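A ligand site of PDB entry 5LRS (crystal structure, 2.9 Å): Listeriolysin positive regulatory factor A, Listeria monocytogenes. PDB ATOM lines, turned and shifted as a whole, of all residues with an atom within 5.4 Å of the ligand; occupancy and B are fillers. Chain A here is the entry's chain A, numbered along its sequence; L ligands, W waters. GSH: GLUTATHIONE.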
ATOM      1  N   GLN A  61     -18.473   7.620   2.497  1.00  0.00           N
ATOM      2  CA  GLN A  61     -17.071   7.934   2.248  1.00  0.00           C
ATOM      3  C   GLN A  61     -16.497   8.659   3.450  1.00  0.00           C
ATOM      4  O   GLN A  61     -17.223   8.949   4.404  1.00  0.00           O
ATOM      5  CB  GLN A  61     -16.915   8.798   0.986  1.00  0.00           C
ATOM      6  CG  GLN A  61     -17.717  10.076   1.006  1.00  0.00           C
ATOM      7  CD  GLN A  61     -17.590  10.861  -0.285  1.00  0.00           C
ATOM      8  OE1 GLN A  61     -18.270  10.563  -1.269  1.00  0.00           O
ATOM      9  NE2 GLN A  61     -16.736  11.876  -0.299  1.00  0.00           N
ATOM     10  N   TYR A  62     -15.198   8.941   3.415  1.00  0.00           N
ATOM     11  CA  TYR A  62     -14.536   9.754   4.432  1.00  0.00           C
ATOM     12  C   TYR A  62     -14.181  11.110   3.848  1.00  0.00           C
ATOM     13  O   TYR A  62     -14.250  11.344   2.638  1.00  0.00           O
ATOM     14  CB  TYR A  62     -13.272   9.065   4.962  1.00  0.00           C
ATOM     15  CG  TYR A  62     -13.498   7.792   5.740  1.00  0.00           C
ATOM     16  CD1 TYR A  62     -14.761   7.267   5.931  1.00  0.00           C
ATOM     17  CD2 TYR A  62     -12.414   7.103   6.293  1.00  0.00           C
ATOM     18  CE1 TYR A  62     -14.960   6.094   6.645  1.00  0.00           C
ATOM     19  CE2 TYR A  62     -12.600   5.939   7.014  1.00  0.00           C
ATOM     20  CZ  TYR A  62     -13.874   5.434   7.185  1.00  0.00           C
ATOM     21  OH  TYR A  62     -14.050   4.269   7.904  1.00  0.00           O
ATOM     22  N   TYR A  63     -13.772  12.020   4.729  1.00  0.00           N
ATOM     23  CA  TYR A  63     -13.306  13.350   4.341  1.00  0.00           C
ATOM     24  C   TYR A  63     -12.103  13.695   5.206  1.00  0.00           C
ATOM     25  O   TYR A  63     -12.230  13.869   6.418  1.00  0.00           O
ATOM     26  CB  TYR A  63     -14.401  14.404   4.504  1.00  0.00           C
ATOM     27  CG  TYR A  63     -15.398  14.425   3.378  1.00  0.00           C
ATOM     28  CD1 TYR A  63     -15.092  15.038   2.171  1.00  0.00           C
ATOM     29  CD2 TYR A  63     -16.657  13.854   3.521  1.00  0.00           C
ATOM     30  CE1 TYR A  63     -15.998  15.076   1.140  1.00  0.00           C
ATOM     31  CE2 TYR A  63     -17.575  13.884   2.493  1.00  0.00           C
ATOM     32  CZ  TYR A  63     -17.246  14.495   1.302  1.00  0.00           C
ATOM     33  OH  TYR A  63     -18.152  14.524   0.281  1.00  0.00           O
ATOM     34  N   LYS A  64     -10.936  13.799   4.567  1.00  0.00           N
ATOM     35  CA  LYS A  64      -9.702  14.228   5.225  1.00  0.00           C
ATOM     36  C   LYS A  64      -9.384  15.640   4.725  1.00  0.00           C
ATOM     37  O   LYS A  64      -9.119  15.833   3.530  1.00  0.00           O
ATOM     38  CB  LYS A  64      -8.561  13.273   4.923  1.00  0.00           C
ATOM     39  CG  LYS A  64      -7.210  13.704   5.479  1.00  0.00           C
ATOM     40  CD  LYS A  64      -6.103  12.794   4.986  1.00  0.00           C
ATOM     41  CE  LYS A  64      -4.723  13.399   5.226  1.00  0.00           C
ATOM     42  NZ  LYS A  64      -3.699  12.833   4.311  1.00  0.00           N
ATOM     43  N   GLY A  65      -9.413  16.610   5.630  1.00  0.00           N
ATOM     44  CA  GLY A  65      -9.215  17.993   5.246  1.00  0.00           C
ATOM     45  C   GLY A  65      -7.940  18.215   4.456  1.00  0.00           C
ATOM     46  O   GLY A  65      -7.015  17.419   4.547  1.00  0.00           O
ATOM     47  N   ALA A  66      -7.872  19.299   3.671  1.00  0.00           N
ATOM     48  CA  ALA A  66      -8.949  20.277   3.531  1.00  0.00           C
ATOM     49  C   ALA A  66      -9.915  19.858   2.436  1.00  0.00           C
ATOM     50  O   ALA A  66      -9.496  19.372   1.390  1.00  0.00           O
ATOM     51  CB  ALA A  66      -8.378  21.651   3.233  1.00  0.00           C
ATOM     52  N   PHE A  67     -11.209  20.056   2.675  1.00  0.00           N
ATOM     53  CA  PHE A  67     -12.223  19.757   1.660  1.00  0.00           C
ATOM     54  C   PHE A  67     -13.490  20.542   1.999  1.00  0.00           C
ATOM     55  O   PHE A  67     -13.558  21.245   3.014  1.00  0.00           O
ATOM     56  CB  PHE A  67     -12.499  18.253   1.579  1.00  0.00           C
ATOM     57  CG  PHE A  67     -12.805  17.780   0.185  1.00  0.00           C
ATOM     58  CD1 PHE A  67     -11.794  17.622  -0.741  1.00  0.00           C
ATOM     59  CD2 PHE A  67     -14.104  17.483  -0.198  1.00  0.00           C
ATOM     60  CE1 PHE A  67     -12.064  17.187  -2.022  1.00  0.00           C
ATOM     61  CE2 PHE A  67     -14.383  17.049  -1.477  1.00  0.00           C
ATOM     62  CZ  PHE A  67     -13.357  16.901  -2.386  1.00  0.00           C
ATOM     63  N   LYS A 122     -13.953  17.273  -7.875  1.00  0.00           N
ATOM     64  CA  LYS A 122     -13.260  16.131  -7.275  1.00  0.00           C
ATOM     65  C   LYS A 122     -14.245  15.175  -6.630  1.00  0.00           C
ATOM     66  O   LYS A 122     -14.096  13.950  -6.730  1.00  0.00           O
ATOM     67  CB  LYS A 122     -12.233  16.623  -6.258  1.00  0.00           C
ATOM     68  CG  LYS A 122     -11.039  17.368  -6.852  1.00  0.00           C
ATOM     69  CD  LYS A 122     -10.097  17.909  -5.783  1.00  0.00           C
ATOM     70  CE  LYS A 122      -9.384  16.792  -5.026  1.00  0.00           C
ATOM     71  NZ  LYS A 122      -8.412  17.331  -4.023  1.00  0.00           N
ATOM     72  N   GLN A 123     -15.263  15.714  -5.960  1.00  0.00           N
ATOM     73  CA  GLN A 123     -16.327  14.872  -5.412  1.00  0.00           C
ATOM     74  C   GLN A 123     -16.994  14.059  -6.519  1.00  0.00           C
ATOM     75  O   GLN A 123     -17.210  12.857  -6.371  1.00  0.00           O
ATOM     76  CB  GLN A 123     -17.350  15.734  -4.675  1.00  0.00           C
ATOM     77  CG  GLN A 123     -18.513  14.965  -4.064  1.00  0.00           C
ATOM     78  CD  GLN A 123     -18.094  14.081  -2.905  1.00  0.00           C
ATOM     79  OE1 GLN A 123     -17.621  14.577  -1.890  1.00  0.00           O
ATOM     80  NE2 GLN A 123     -18.246  12.773  -3.066  1.00  0.00           N
ATOM     81  N   TYR A 126     -14.680  11.351  -7.940  1.00  0.00           N
ATOM     82  CA  TYR A 126     -14.550  10.336  -6.901  1.00  0.00           C
ATOM     83  C   TYR A 126     -15.762   9.406  -6.901  1.00  0.00           C
ATOM     84  O   TYR A 126     -15.618   8.183  -6.979  1.00  0.00           O
ATOM     85  CB  TYR A 126     -14.389  11.012  -5.538  1.00  0.00           C
ATOM     86  CG  TYR A 126     -14.465  10.052  -4.375  1.00  0.00           C
ATOM     87  CD1 TYR A 126     -13.363   9.290  -4.003  1.00  0.00           C
ATOM     88  CD2 TYR A 126     -15.631   9.919  -3.642  1.00  0.00           C
ATOM     89  CE1 TYR A 126     -13.430   8.420  -2.940  1.00  0.00           C
ATOM     90  CE2 TYR A 126     -15.708   9.041  -2.567  1.00  0.00           C
ATOM     91  CZ  TYR A 126     -14.608   8.296  -2.227  1.00  0.00           C
ATOM     92  OH  TYR A 126     -14.685   7.428  -1.162  1.00  0.00           O
ATOM     93  N   LYS A 130     -15.727   5.405  -7.863  1.00  0.00           N
ATOM     94  CA  LYS A 130     -16.147   4.475  -6.823  1.00  0.00           C
ATOM     95  C   LYS A 130     -17.331   3.640  -7.304  1.00  0.00           C
ATOM     96  O   LYS A 130     -17.344   2.417  -7.151  1.00  0.00           O
ATOM     97  CB  LYS A 130     -16.500   5.242  -5.548  1.00  0.00           C
ATOM     98  CG  LYS A 130     -16.585   4.385  -4.299  1.00  0.00           C
ATOM     99  CD  LYS A 130     -16.646   5.255  -3.054  1.00  0.00           C
ATOM    100  CE  LYS A 130     -16.588   4.429  -1.784  1.00  0.00           C
ATOM    101  NZ  LYS A 130     -16.576   5.293  -0.582  1.00  0.00           N
ATOM    102  N   GLN A 146     -12.276   0.101  -1.497  1.00  0.00           N
ATOM    103  CA  GLN A 146     -12.155   0.823  -0.233  1.00  0.00           C
ATOM    104  C   GLN A 146     -10.733   0.731   0.302  1.00  0.00           C
ATOM    105  O   GLN A 146     -10.148   1.735   0.725  1.00  0.00           O
ATOM    106  CB  GLN A 146     -13.151   0.276   0.778  1.00  0.00           C
ATOM    107  CG  GLN A 146     -13.186   1.048   2.098  1.00  0.00           C
ATOM    108  CD  GLN A 146     -13.602   2.489   1.922  1.00  0.00           C
ATOM    109  OE1 GLN A 146     -14.091   2.885   0.857  1.00  0.00           O
ATOM    110  NE2 GLN A 146     -13.421   3.289   2.966  1.00  0.00           N
ATOM    111  N   ILE A 149      -8.534   3.075  -1.544  1.00  0.00           N
ATOM    112  CA  ILE A 149      -8.767   4.452  -1.116  1.00  0.00           C
ATOM    113  C   ILE A 149      -8.048   4.728   0.189  1.00  0.00           C
ATOM    114  O   ILE A 149      -7.246   5.674   0.302  1.00  0.00           O
ATOM    115  CB  ILE A 149     -10.285   4.713  -0.994  1.00  0.00           C
ATOM    116  CG1 ILE A 149     -10.976   4.519  -2.341  1.00  0.00           C
ATOM    117  CG2 ILE A 149     -10.547   6.116  -0.460  1.00  0.00           C
ATOM    118  CD1 ILE A 149     -12.477   4.447  -2.256  1.00  0.00           C
ATOM    119  N   LEU A 150      -8.309   3.905   1.212  1.00  0.00           N
ATOM    120  CA  LEU A 150      -7.654   4.066   2.497  1.00  0.00           C
ATOM    121  C   LEU A 150      -6.139   4.029   2.368  1.00  0.00           C
ATOM    122  O   LEU A 150      -5.430   4.723   3.110  1.00  0.00           O
ATOM    123  CB  LEU A 150      -8.136   2.976   3.459  1.00  0.00           C
ATOM    124  CG  LEU A 150      -9.651   2.922   3.688  1.00  0.00           C
ATOM    125  CD1 LEU A 150     -10.033   1.684   4.481  1.00  0.00           C
ATOM    126  CD2 LEU A 150     -10.136   4.176   4.397  1.00  0.00           C
ATOM    127  N   VAL A 153      -5.101   7.604   0.713  1.00  0.00           N
ATOM    128  CA  VAL A 153      -5.331   8.800   1.533  1.00  0.00           C
ATOM    129  C   VAL A 153      -4.654   8.671   2.889  1.00  0.00           C
ATOM    130  O   VAL A 153      -4.026   9.624   3.370  1.00  0.00           O
ATOM    131  CB  VAL A 153      -6.848   9.044   1.687  1.00  0.00           C
ATOM    132  CG1 VAL A 153      -7.100  10.329   2.463  1.00  0.00           C
ATOM    133  CG2 VAL A 153      -7.518   9.100   0.325  1.00  0.00           C
ATOM    134  N   TYR A 154      -4.742   7.502   3.521  1.00  0.00           N
ATOM    135  CA  TYR A 154      -4.249   7.311   4.885  1.00  0.00           C
ATOM    136  C   TYR A 154      -3.107   6.305   4.954  1.00  0.00           C
ATOM    137  O   TYR A 154      -2.819   5.790   6.045  1.00  0.00           O
ATOM    138  CB  TYR A 154      -5.397   6.878   5.792  1.00  0.00           C
ATOM    139  CG  TYR A 154      -6.684   7.633   5.556  1.00  0.00           C
ATOM    140  CD1 TYR A 154      -6.835   8.938   5.996  1.00  0.00           C
ATOM    141  CD2 TYR A 154      -7.734   7.049   4.867  1.00  0.00           C
ATOM    142  CE1 TYR A 154      -8.005   9.635   5.774  1.00  0.00           C
ATOM    143  CE2 TYR A 154      -8.906   7.737   4.646  1.00  0.00           C
ATOM    144  CZ  TYR A 154      -9.038   9.029   5.094  1.00  0.00           C
ATOM    145  OH  TYR A 154     -10.210   9.717   4.873  1.00  0.00           O
ATOM    146  N   TRP A 224      -8.412   7.827 -10.706  1.00  0.00           N
ATOM    147  CA  TRP A 224      -8.850   9.056 -10.054  1.00  0.00           C
ATOM    148  C   TRP A 224      -7.722   9.654  -9.227  1.00  0.00           C
ATOM    149  O   TRP A 224      -7.443  10.854  -9.305  1.00  0.00           O
ATOM    150  CB  TRP A 224     -10.066   8.784  -9.169  1.00  0.00           C
ATOM    151  CG  TRP A 224     -10.510  10.005  -8.424  1.00  0.00           C
ATOM    152  CD1 TRP A 224     -11.211  11.058  -8.913  1.00  0.00           C
ATOM    153  CD2 TRP A 224     -10.257  10.302  -7.036  1.00  0.00           C
ATOM    154  NE1 TRP A 224     -11.418  11.993  -7.933  1.00  0.00           N
ATOM    155  CE2 TRP A 224     -10.847  11.554  -6.766  1.00  0.00           C
ATOM    156  CE3 TRP A 224      -9.607   9.622  -6.007  1.00  0.00           C
ATOM    157  CZ2 TRP A 224     -10.801  12.144  -5.508  1.00  0.00           C
ATOM    158  CZ3 TRP A 224      -9.563  10.211  -4.758  1.00  0.00           C
ATOM    159  CH2 TRP A 224     -10.149  11.459  -4.520  1.00  0.00           C
ATOM    160  N   PHE A 225      -7.070   8.829  -8.401  1.00  0.00           N
ATOM    161  CA  PHE A 225      -5.954   9.333  -7.605  1.00  0.00           C
ATOM    162  C   PHE A 225      -4.837   9.864  -8.494  1.00  0.00           C
ATOM    163  O   PHE A 225      -4.172  10.840  -8.124  1.00  0.00           O
ATOM    164  CB  PHE A 225      -5.432   8.245  -6.672  1.00  0.00           C
ATOM    165  CG  PHE A 225      -6.287   8.023  -5.459  1.00  0.00           C
ATOM    166  CD1 PHE A 225      -6.203   8.874  -4.371  1.00  0.00           C
ATOM    167  CD2 PHE A 225      -7.174   6.966  -5.415  1.00  0.00           C
ATOM    168  CE1 PHE A 225      -6.986   8.682  -3.255  1.00  0.00           C
ATOM    169  CE2 PHE A 225      -7.968   6.765  -4.296  1.00  0.00           C
ATOM    170  CZ  PHE A 225      -7.875   7.623  -3.220  1.00  0.00           C
ATOM    171  N   CYS A 229      -5.763  13.585  -7.275  1.00  0.00           N
ATOM    172  CA  CYS A 229      -4.839  13.728  -6.150  1.00  0.00           C
ATOM    173  C   CYS A 229      -3.470  13.193  -6.568  1.00  0.00           C
ATOM    174  O   CYS A 229      -2.983  12.202  -6.004  1.00  0.00           O
ATOM    175  CB  CYS A 229      -5.357  12.999  -4.915  1.00  0.00           C
ATOM    176  SG  CYS A 229      -6.985  13.560  -4.349  1.00  0.00           S
ATOM    177  N   THR A 232      -0.797  12.510  -3.714  1.00  0.00           N
ATOM    178  CA  THR A 232      -1.133  11.300  -2.983  1.00  0.00           C
ATOM    179  C   THR A 232      -0.840  10.054  -3.800  1.00  0.00           C
ATOM    180  O   THR A 232      -0.485   9.012  -3.239  1.00  0.00           O
ATOM    181  CB  THR A 232      -2.611  11.342  -2.575  1.00  0.00           C
ATOM    182  OG1 THR A 232      -2.923  12.631  -2.033  1.00  0.00           O
ATOM    183  CG2 THR A 232      -2.912  10.272  -1.535  1.00  0.00           C
HETATM  184  N1  GSH L   1      -7.790  17.123   1.143  1.00  0.00           N
HETATM  185  CA1 GSH L   1      -7.422  15.926   0.410  1.00  0.00           C
HETATM  186  C1  GSH L   1      -7.360  16.240  -1.085  1.00  0.00           C
HETATM  187  O11 GSH L   1      -6.707  15.463  -1.844  1.00  0.00           O
HETATM  188  O12 GSH L   1      -7.954  17.262  -1.520  1.00  0.00           O
HETATM  189  CB1 GSH L   1      -8.459  14.831   0.647  1.00  0.00           C
HETATM  190  CG1 GSH L   1      -9.894  15.257   0.353  1.00  0.00           C
HETATM  191  CD1 GSH L   1     -10.868  14.084   0.432  1.00  0.00           C
HETATM  192  OE1 GSH L   1     -11.127  13.563   1.521  1.00  0.00           O
HETATM  193  N2  GSH L   1     -11.400  13.673  -0.722  1.00  0.00           N
HETATM  194  CA2 GSH L   1     -12.327  12.555  -0.727  1.00  0.00           C
HETATM  195  C2  GSH L   1     -11.543  11.299  -0.389  1.00  0.00           C
HETATM  196  O2  GSH L   1     -10.418  11.132  -0.865  1.00  0.00           O
HETATM  197  CB2 GSH L   1     -12.988  12.375  -2.091  1.00  0.00           C
HETATM  198  SG2 GSH L   1     -14.271  13.606  -2.439  1.00  0.00           S
HETATM  199  N3  GSH L   1     -12.135  10.433   0.422  1.00  0.00           N
HETATM  200  CA3 GSH L   1     -11.444   9.205   0.795  1.00  0.00           C
HETATM  201  C3  GSH L   1     -12.376   8.206   1.495  1.00  0.00           C
HETATM  202  O31 GSH L   1     -13.538   8.071   1.024  1.00  0.00           O
HETATM  203  O32 GSH L   1     -11.919   7.582   2.483  1.00  0.00           O
HETATM  204  O   HOH W   1     -13.878   5.751   2.398  1.00  0.00           O
HETATM  205  O   HOH W   2      -5.670  18.589   2.014  1.00  0.00           O
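Tyr 63 touches the ligand (CA to OE1, 3.6 Å). Gly 65 touches the ligand (C to N1, 3.5 Å). CD1 of Phe 67 touches CG1 of the ligand, 3.2 Å away. Ile 149 touches the ligand (CG2 to C3, 3.4 Å). Val 153 touches the ligand (CG2 to O2, 3.7 Å). OH of Tyr 154 touches O32 of the ligand, at 3.6 Å. Trp 224 touches the ligand. Hydrophobic or aromatic side chains within 4 Å of the ligand: Tyr 62, Phe 67, Tyr 126, Ile 149, Val 153, Tyr 154 and Trp 224. 15 residues have an atom within 4 Å of the ligand: Gln 61, Tyr 62, Tyr 63, Lys 64, Gly 65, Ala 66, Phe 67, Lys 122, Gln 123, Tyr 126, Ile 149, Val 153, Tyr 154, Trp 224 and Cys 229. The nearest printed residue that does not touch the ligand is Leu 150 (4.3 Å).
Water W1 lies within hydrogen-bond range of NE2 of Gln 146 and O32 of the ligand. Water W2 lies within hydrogen-bond range of N1 of the ligand (2.7 Å), N of Ala 66 (2.8 Å) and O of Gly 65 (3.1 Å).
O of Val 153 is in hydrogen-bond range of NZ of Lys 64 (3.4 Å). The side-chain amide oxygen of Gln 61 lies within hydrogen-bond range of the side-chain amide nitrogen of Gln 123, at 2.8 Å. The side-chain amino group of Lys 130 is in hydrogen-bond range of the side-chain hydroxyl of Tyr 126 (2.9 Å). The side-chain hydroxyl (OH) of Tyr 63 lies within hydrogen-bond range of the side-chain amide nitrogen (NE2) of Gln 61, at 3.1 Å.
The backbone NH of Ala 66 lies close to a nitrogen (N1) of the ligand (3.3 Å). The backbone NH of Tyr 62 is in hydrogen-bond range of an oxygen (O31) of the ligand, at 3.0 Å. The backbone carbonyl oxygen of Tyr 62 is in hydrogen-bond range of a nitrogen (N3) of the ligand, at 3.2 Å. The side-chain amino group (NZ) of Lys 122 lies within salt-bridge range of an oxygen (O12) of the ligand (2.5 Å). A sulfur (SG2) of the ligand lies close to the side-chain amide oxygen (OE1) of Gln 123 (3.5 Å). A nitrogen (N1) of the ligand is in hydrogen-bond range of the backbone carbonyl oxygen (O) of Ala 66 (2.8 Å). O of Lys 64 sits at hydrogen-bond distance from N1 of the ligand, 3.0 Å away. The side-chain sulfur (SG) of Cys 229 sits at hydrogen-bond distance from an oxygen (O11) of the ligand (3.2 Å). The side-chain amide nitrogen (NE2) of Gln 61 sits close to a sulfur (SG2) of the ligand. OH of Tyr 126 sits at hydrogen-bond distance from O31 of the ligand. The backbone NH (N) of Lys 64 is in hydrogen-bond range of an oxygen (OE1) of the ligand (3.1 Å).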
